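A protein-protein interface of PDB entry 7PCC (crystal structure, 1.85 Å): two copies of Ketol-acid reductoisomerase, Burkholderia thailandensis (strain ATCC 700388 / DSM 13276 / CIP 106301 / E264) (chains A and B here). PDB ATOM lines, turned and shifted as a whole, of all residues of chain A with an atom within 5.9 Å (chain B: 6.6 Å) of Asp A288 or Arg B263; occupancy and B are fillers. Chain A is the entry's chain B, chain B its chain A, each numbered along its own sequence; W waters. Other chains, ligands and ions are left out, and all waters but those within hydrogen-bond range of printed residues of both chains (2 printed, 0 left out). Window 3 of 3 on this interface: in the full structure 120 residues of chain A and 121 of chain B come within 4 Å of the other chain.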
ATOM      1  N   GLN A 196       0.030  -5.213 -14.929  1.00  0.00           N
ATOM      2  CA  GLN A 196      -1.003  -6.113 -15.514  1.00  0.00           C
ATOM      3  C   GLN A 196      -2.412  -5.528 -15.365  1.00  0.00           C
ATOM      4  O   GLN A 196      -3.226  -5.794 -16.260  1.00  0.00           O
ATOM      5  CB  GLN A 196      -0.922  -7.503 -14.884  1.00  0.00           C
ATOM      6  CG  GLN A 196       0.248  -8.321 -15.410  1.00  0.00           C
ATOM      7  CD  GLN A 196       0.470  -9.606 -14.652  1.00  0.00           C
ATOM      8  OE1 GLN A 196      -0.463 -10.358 -14.380  1.00  0.00           O
ATOM      9  NE2 GLN A 196       1.724  -9.877 -14.323  1.00  0.00           N
ATOM     10  N   ASP A 282      -5.170 -12.538  -8.316  1.00  0.00           N
ATOM     11  CA  ASP A 282      -5.341 -14.012  -8.180  1.00  0.00           C
ATOM     12  C   ASP A 282      -4.386 -14.727  -9.142  1.00  0.00           C
ATOM     13  O   ASP A 282      -3.716 -15.686  -8.703  1.00  0.00           O
ATOM     14  CB  ASP A 282      -6.791 -14.438  -8.420  1.00  0.00           C
ATOM     15  CG  ASP A 282      -7.757 -14.023  -7.323  1.00  0.00           C
ATOM     16  OD1 ASP A 282      -7.294 -13.454  -6.316  1.00  0.00           O
ATOM     17  OD2 ASP A 282      -8.967 -14.273  -7.482  1.00  0.00           O
ATOM     18  N   GLN A 283      -4.319 -14.274 -10.399  1.00  0.00           N
ATOM     19  CA  GLN A 283      -3.417 -14.841 -11.439  1.00  0.00           C
ATOM     20  C   GLN A 283      -1.957 -14.639 -11.018  1.00  0.00           C
ATOM     21  O   GLN A 283      -1.145 -15.561 -11.224  1.00  0.00           O
ATOM     22  CB  GLN A 283      -3.639 -14.170 -12.792  1.00  0.00           C
ATOM     23  CG  GLN A 283      -4.924 -14.579 -13.488  1.00  0.00           C
ATOM     24  CD  GLN A 283      -5.034 -13.873 -14.816  1.00  0.00           C
ATOM     25  OE1 GLN A 283      -4.452 -12.809 -15.016  1.00  0.00           O
ATOM     26  NE2 GLN A 283      -5.767 -14.468 -15.742  1.00  0.00           N
ATOM     27  N   ILE A 284      -1.640 -13.463 -10.476  1.00  0.00           N
ATOM     28  CA  ILE A 284      -0.262 -13.081 -10.051  1.00  0.00           C
ATOM     29  C   ILE A 284       0.150 -13.953  -8.856  1.00  0.00           C
ATOM     30  O   ILE A 284       1.254 -14.528  -8.898  1.00  0.00           O
ATOM     31  CB  ILE A 284      -0.193 -11.570  -9.742  1.00  0.00           C
ATOM     32  CG1 ILE A 284      -0.236 -10.736 -11.026  1.00  0.00           C
ATOM     33  CG2 ILE A 284       1.029 -11.238  -8.897  1.00  0.00           C
ATOM     34  CD1 ILE A 284      -0.510  -9.261 -10.805  1.00  0.00           C
ATOM     35  N   GLY A 286      -1.198 -16.791  -7.557  1.00  0.00           N
ATOM     36  CA  GLY A 286      -1.531 -18.230  -7.577  1.00  0.00           C
ATOM     37  C   GLY A 286      -0.628 -19.066  -8.474  1.00  0.00           C
ATOM     38  O   GLY A 286      -0.671 -20.301  -8.327  1.00  0.00           O
ATOM     39  N   GLY A 287       0.135 -18.445  -9.386  1.00  0.00           N
ATOM     40  CA  GLY A 287       1.089 -19.140 -10.278  1.00  0.00           C
ATOM     41  C   GLY A 287       0.675 -19.113 -11.745  1.00  0.00           C
ATOM     42  O   GLY A 287       1.499 -19.519 -12.593  1.00  0.00           O
ATOM     43  N   ASP A 288      -0.547 -18.664 -12.045  1.00  0.00           N
ATOM     44  CA  ASP A 288      -1.104 -18.563 -13.423  1.00  0.00           C
ATOM     45  C   ASP A 288      -0.176 -17.691 -14.283  1.00  0.00           C
ATOM     46  O   ASP A 288       0.256 -18.165 -15.354  1.00  0.00           O
ATOM     47  CB  ASP A 288      -2.535 -18.019 -13.390  1.00  0.00           C
ATOM     48  CG  ASP A 288      -3.211 -17.926 -14.747  1.00  0.00           C
ATOM     49  OD1 ASP A 288      -2.636 -17.290 -15.647  1.00  0.00           O
ATOM     50  OD2 ASP A 288      -4.317 -18.483 -14.888  1.00  0.00           O
ATOM     51  N   PHE A 289       0.120 -16.466 -13.843  1.00  0.00           N
ATOM     52  CA  PHE A 289       0.978 -15.515 -14.599  1.00  0.00           C
ATOM     53  C   PHE A 289       2.390 -16.089 -14.754  1.00  0.00           C
ATOM     54  O   PHE A 289       2.936 -16.043 -15.867  1.00  0.00           O
ATOM     55  CB  PHE A 289       1.077 -14.140 -13.938  1.00  0.00           C
ATOM     56  CG  PHE A 289       2.034 -13.239 -14.672  1.00  0.00           C
ATOM     57  CD1 PHE A 289       1.782 -12.876 -15.988  1.00  0.00           C
ATOM     58  CD2 PHE A 289       3.215 -12.812 -14.082  1.00  0.00           C
ATOM     59  CE1 PHE A 289       2.674 -12.075 -16.686  1.00  0.00           C
ATOM     60  CE2 PHE A 289       4.102 -12.007 -14.782  1.00  0.00           C
ATOM     61  CZ  PHE A 289       3.829 -11.637 -16.080  1.00  0.00           C
ATOM     62  N   SER A 290       2.969 -16.587 -13.660  1.00  0.00           N
ATOM     63  CA  SER A 290       4.328 -17.190 -13.617  1.00  0.00           C
ATOM     64  C   SER A 290       4.492 -18.188 -14.772  1.00  0.00           C
ATOM     65  O   SER A 290       5.520 -18.116 -15.474  1.00  0.00           O
ATOM     66  CB  SER A 290       4.588 -17.828 -12.274  1.00  0.00           C
ATOM     67  OG  SER A 290       5.759 -18.629 -12.312  1.00  0.00           O
ATOM     68  N   ALA A 291       3.503 -19.060 -14.979  1.00  0.00           N
ATOM     69  CA  ALA A 291       3.478 -20.088 -16.048  1.00  0.00           C
ATOM     70  C   ALA A 291       3.373 -19.416 -17.425  1.00  0.00           C
ATOM     71  O   ALA A 291       4.096 -19.847 -18.348  1.00  0.00           O
ATOM     72  CB  ALA A 291       2.337 -21.052 -15.809  1.00  0.00           C
ATOM     73  N   TYR A 292       2.508 -18.401 -17.550  1.00  0.00           N
ATOM     74  CA  TYR A 292       2.263 -17.616 -18.790  1.00  0.00           C
ATOM     75  C   TYR A 292       3.558 -16.908 -19.211  1.00  0.00           C
ATOM     76  O   TYR A 292       3.864 -16.893 -20.416  1.00  0.00           O
ATOM     77  CB  TYR A 292       1.106 -16.634 -18.576  1.00  0.00           C
ATOM     78  CG  TYR A 292       0.793 -15.717 -19.734  1.00  0.00           C
ATOM     79  CD1 TYR A 292       1.346 -14.448 -19.811  1.00  0.00           C
ATOM     80  CD2 TYR A 292      -0.080 -16.102 -20.740  1.00  0.00           C
ATOM     81  CE1 TYR A 292       1.054 -13.592 -20.862  1.00  0.00           C
ATOM     82  CE2 TYR A 292      -0.382 -15.258 -21.798  1.00  0.00           C
ATOM     83  CZ  TYR A 292       0.187 -13.998 -21.860  1.00  0.00           C
ATOM     84  OH  TYR A 292      -0.106 -13.159 -22.898  1.00  0.00           O
ATOM     85  N   LEU A 293       4.306 -16.358 -18.250  1.00  0.00           N
ATOM     86  CA  LEU A 293       5.569 -15.613 -18.512  1.00  0.00           C
ATOM     87  C   LEU A 293       6.643 -16.576 -19.035  1.00  0.00           C
ATOM     88  O   LEU A 293       7.311 -16.223 -20.026  1.00  0.00           O
ATOM     89  CB  LEU A 293       6.028 -14.908 -17.231  1.00  0.00           C
ATOM     90  CG  LEU A 293       7.439 -14.321 -17.268  1.00  0.00           C
ATOM     91  CD1 LEU A 293       7.587 -13.310 -18.399  1.00  0.00           C
ATOM     92  CD2 LEU A 293       7.799 -13.687 -15.932  1.00  0.00           C
ATOM     93  N   GLN B 258       6.361  -6.051 -19.924  1.00  0.00           N
ATOM     94  CA  GLN B 258       5.787  -6.062 -21.297  1.00  0.00           C
ATOM     95  C   GLN B 258       4.849  -7.267 -21.465  1.00  0.00           C
ATOM     96  O   GLN B 258       3.756  -7.085 -22.028  1.00  0.00           O
ATOM     97  CB  GLN B 258       6.901  -6.089 -22.340  1.00  0.00           C
ATOM     98  CG  GLN B 258       7.802  -4.865 -22.294  1.00  0.00           C
ATOM     99  CD  GLN B 258       8.534  -4.631 -23.591  1.00  0.00           C
ATOM    100  OE1 GLN B 258       8.007  -4.867 -24.680  1.00  0.00           O
ATOM    101  NE2 GLN B 258       9.753  -4.133 -23.484  1.00  0.00           N
ATOM    102  N   VAL B 259       5.253  -8.451 -20.998  1.00  0.00           N
ATOM    103  CA  VAL B 259       4.443  -9.698 -21.139  1.00  0.00           C
ATOM    104  C   VAL B 259       3.123  -9.509 -20.380  1.00  0.00           C
ATOM    105  O   VAL B 259       2.064  -9.826 -20.956  1.00  0.00           O
ATOM    106  CB  VAL B 259       5.211 -10.950 -20.672  1.00  0.00           C
ATOM    107  CG1 VAL B 259       4.290 -12.150 -20.494  1.00  0.00           C
ATOM    108  CG2 VAL B 259       6.344 -11.300 -21.624  1.00  0.00           C
ATOM    109  N   GLY B 260       3.186  -9.005 -19.142  1.00  0.00           N
ATOM    110  CA  GLY B 260       2.013  -8.758 -18.279  1.00  0.00           C
ATOM    111  C   GLY B 260       1.090  -7.696 -18.859  1.00  0.00           C
ATOM    112  O   GLY B 260      -0.135  -7.925 -18.900  1.00  0.00           O
ATOM    113  N   TYR B 261       1.659  -6.569 -19.290  1.00  0.00           N
ATOM    114  CA  TYR B 261       0.940  -5.429 -19.919  1.00  0.00           C
ATOM    115  C   TYR B 261       0.122  -5.922 -21.117  1.00  0.00           C
ATOM    116  O   TYR B 261      -1.082  -5.606 -21.200  1.00  0.00           O
ATOM    117  CB  TYR B 261       1.937  -4.356 -20.350  1.00  0.00           C
ATOM    118  CG  TYR B 261       1.355  -3.171 -21.079  1.00  0.00           C
ATOM    119  CD1 TYR B 261       1.368  -3.104 -22.465  1.00  0.00           C
ATOM    120  CD2 TYR B 261       0.834  -2.092 -20.384  1.00  0.00           C
ATOM    121  CE1 TYR B 261       0.856  -2.008 -23.142  1.00  0.00           C
ATOM    122  CE2 TYR B 261       0.322  -0.986 -21.044  1.00  0.00           C
ATOM    123  CZ  TYR B 261       0.339  -0.941 -22.427  1.00  0.00           C
ATOM    124  OH  TYR B 261      -0.160   0.150 -23.074  1.00  0.00           O
ATOM    125  N   HIS B 262       0.761  -6.681 -22.011  1.00  0.00           N
ATOM    126  CA  HIS B 262       0.170  -7.140 -23.296  1.00  0.00           C
ATOM    127  C   HIS B 262      -0.858  -8.245 -23.046  1.00  0.00           C
ATOM    128  O   HIS B 262      -1.679  -8.476 -23.942  1.00  0.00           O
ATOM    129  CB  HIS B 262       1.263  -7.548 -24.293  1.00  0.00           C
ATOM    130  CG  HIS B 262       1.871  -6.372 -24.980  1.00  0.00           C
ATOM    131  ND1 HIS B 262       1.124  -5.527 -25.779  1.00  0.00           N
ATOM    132  CD2 HIS B 262       3.126  -5.874 -24.963  1.00  0.00           C
ATOM    133  CE1 HIS B 262       1.899  -4.567 -26.236  1.00  0.00           C
ATOM    134  NE2 HIS B 262       3.132  -4.757 -25.748  1.00  0.00           N
ATOM    135  N   ARG B 263      -0.834  -8.886 -21.874  1.00  0.00           N
ATOM    136  CA  ARG B 263      -1.846  -9.908 -21.502  1.00  0.00           C
ATOM    137  C   ARG B 263      -3.209  -9.235 -21.323  1.00  0.00           C
ATOM    138  O   ARG B 263      -4.218  -9.861 -21.692  1.00  0.00           O
ATOM    139  CB  ARG B 263      -1.468 -10.660 -20.223  1.00  0.00           C
ATOM    140  CG  ARG B 263      -2.328 -11.895 -19.992  1.00  0.00           C
ATOM    141  CD  ARG B 263      -1.898 -12.728 -18.804  1.00  0.00           C
ATOM    142  NE  ARG B 263      -2.518 -14.043 -18.847  1.00  0.00           N
ATOM    143  CZ  ARG B 263      -2.438 -14.961 -17.888  1.00  0.00           C
ATOM    144  NH1 ARG B 263      -1.765 -14.717 -16.774  1.00  0.00           N
ATOM    145  NH2 ARG B 263      -3.040 -16.127 -18.050  1.00  0.00           N
ATOM    146  N   TRP B 264      -3.240  -8.016 -20.774  1.00  0.00           N
ATOM    147  CA  TRP B 264      -4.499  -7.338 -20.363  1.00  0.00           C
ATOM    148  C   TRP B 264      -4.793  -6.102 -21.216  1.00  0.00           C
ATOM    149  O   TRP B 264      -5.936  -5.624 -21.146  1.00  0.00           O
ATOM    150  CB  TRP B 264      -4.459  -7.025 -18.865  1.00  0.00           C
ATOM    151  CG  TRP B 264      -4.638  -8.269 -18.054  1.00  0.00           C
ATOM    152  CD1 TRP B 264      -3.685  -8.954 -17.360  1.00  0.00           C
ATOM    153  CD2 TRP B 264      -5.853  -9.026 -17.925  1.00  0.00           C
ATOM    154  NE1 TRP B 264      -4.229 -10.070 -16.785  1.00  0.00           N
ATOM    155  CE2 TRP B 264      -5.558 -10.143 -17.117  1.00  0.00           C
ATOM    156  CE3 TRP B 264      -7.158  -8.863 -18.405  1.00  0.00           C
ATOM    157  CZ2 TRP B 264      -6.527 -11.082 -16.770  1.00  0.00           C
ATOM    158  CZ3 TRP B 264      -8.114  -9.800 -18.071  1.00  0.00           C
ATOM    159  CH2 TRP B 264      -7.800 -10.891 -17.261  1.00  0.00           C
ATOM    160  N   ARG B 265      -3.828  -5.626 -22.009  1.00  0.00           N
ATOM    161  CA  ARG B 265      -4.013  -4.452 -22.901  1.00  0.00           C
ATOM    162  C   ARG B 265      -5.225  -4.717 -23.803  1.00  0.00           C
ATOM    163  O   ARG B 265      -5.252  -5.774 -24.456  1.00  0.00           O
ATOM    164  CB  ARG B 265      -2.738  -4.186 -23.708  1.00  0.00           C
ATOM    165  CG  ARG B 265      -2.832  -3.004 -24.659  1.00  0.00           C
ATOM    166  CD  ARG B 265      -2.898  -1.652 -23.974  1.00  0.00           C
ATOM    167  NE  ARG B 265      -2.777  -0.627 -25.000  1.00  0.00           N
ATOM    168  CZ  ARG B 265      -3.792  -0.063 -25.650  1.00  0.00           C
ATOM    169  NH1 ARG B 265      -5.045  -0.372 -25.354  1.00  0.00           N
ATOM    170  NH2 ARG B 265      -3.545   0.831 -26.590  1.00  0.00           N
ATOM    171  N   ARG B 267      -8.264  -5.334 -22.813  1.00  0.00           N
ATOM    172  CA  ARG B 267      -9.166  -6.343 -22.187  1.00  0.00           C
ATOM    173  C   ARG B 267      -9.634  -5.901 -20.789  1.00  0.00           C
ATOM    174  O   ARG B 267     -10.381  -6.680 -20.170  1.00  0.00           O
ATOM    175  CB  ARG B 267      -8.460  -7.701 -22.091  1.00  0.00           C
ATOM    176  CG  ARG B 267      -7.856  -8.191 -23.401  1.00  0.00           C
ATOM    177  CD  ARG B 267      -7.615  -9.692 -23.452  1.00  0.00           C
ATOM    178  NE  ARG B 267      -6.775 -10.200 -22.369  1.00  0.00           N
ATOM    179  CZ  ARG B 267      -7.143 -11.087 -21.435  1.00  0.00           C
ATOM    180  NH1 ARG B 267      -8.362 -11.605 -21.422  1.00  0.00           N
ATOM    181  NH2 ARG B 267      -6.275 -11.461 -20.508  1.00  0.00           N
HETATM  182  O   HOH W   1       1.243 -10.947 -23.071  1.00  0.00           O
HETATM  183  O   HOH W   2      -2.014 -12.212 -15.268  1.00  0.00           O
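Among the printed residues, merely in contact across the chains: Gln A196 with Gly B260 (3.4 Å), Gln A196 with Trp B264 (3.1 Å), Gln A283 with Arg B263 (3.7 Å), Phe A289 with Gly B260 (3.7 Å), Phe A289 with Arg B263 (3.6 Å), Tyr A292 with Val B259 (3.6 Å), Tyr A292 with Arg B263 (3.7 Å) and Leu A293 with Val B259 (3.998 Å).
No position is printed for both chains.
Arg B263 touches four residues of chain A.
Of the printed residues of chain B, Tyr A292 touches Val B259 and Arg B263.
Of the printed residues of chain B, Leu A293 touches Val B259.
Ser A290 touches none of the printed residues of chain B.
The nearest printed residue of chain B that does not touch Asp A288 is Trp B264 (7.4 Å).
The nearest printed residue of chain B that does not touch Tyr A292 is His B262 (5.0 Å).
Water W2 lies within hydrogen-bond range of OE1 of Gln A283 (2.5 Å), OE1 of Gln A196 (2.6 Å), NH1 of Arg B263 (2.9 Å) and NE1 of Trp B264 (3.4 Å).
Water W1 lies within hydrogen-bond range of the backbone carbonyl oxygen (O) of Val B259 (2.5 Å), the side-chain hydroxyl (OH) of Tyr A292 (2.6 Å) and the backbone NH (N) of Arg B263 (3.2 Å).
The guanidinium group (NE) of Arg B267 lies within hydrogen-bond range of the backbone carbonyl oxygen (O) of Arg B263.
The backbone carbonyl oxygen of Gln A283 sits at hydrogen-bond distance from the backbone NH of Asp A288, 3.3 Å away.
O of Gln A283 sits at hydrogen-bond distance from N of Phe A289 (3.0 Å).
Of the 9 printed residues of chain B, 4 touch a printed residue of chain A.
Printed residues of chain B that touch a printed residue of chain A: Val B259, Gly B260, Arg B263 and Trp B264.
Printed residues of chain A that touch a printed residue of chain B: Gln A196, Gln A283, Asp A288, Phe A289, Tyr A292 and Leu A293.
Hydrophobic or aromatic side chains of chain A that line the printed part of chain B: Phe A289, Tyr A292 and Leu A293.
Along chain A the printed residues that touch a printed residue of chain B span positions 196 to 293.
The guanidinium group (NH2) of Arg B263 is in salt-bridge range of the side-chain carboxylate (OD1) of Asp A288 (2.7 Å).
The side-chain amide oxygen (OE1) of Gln A283 lies close to the indole nitrogen (NE1) of Trp B264.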
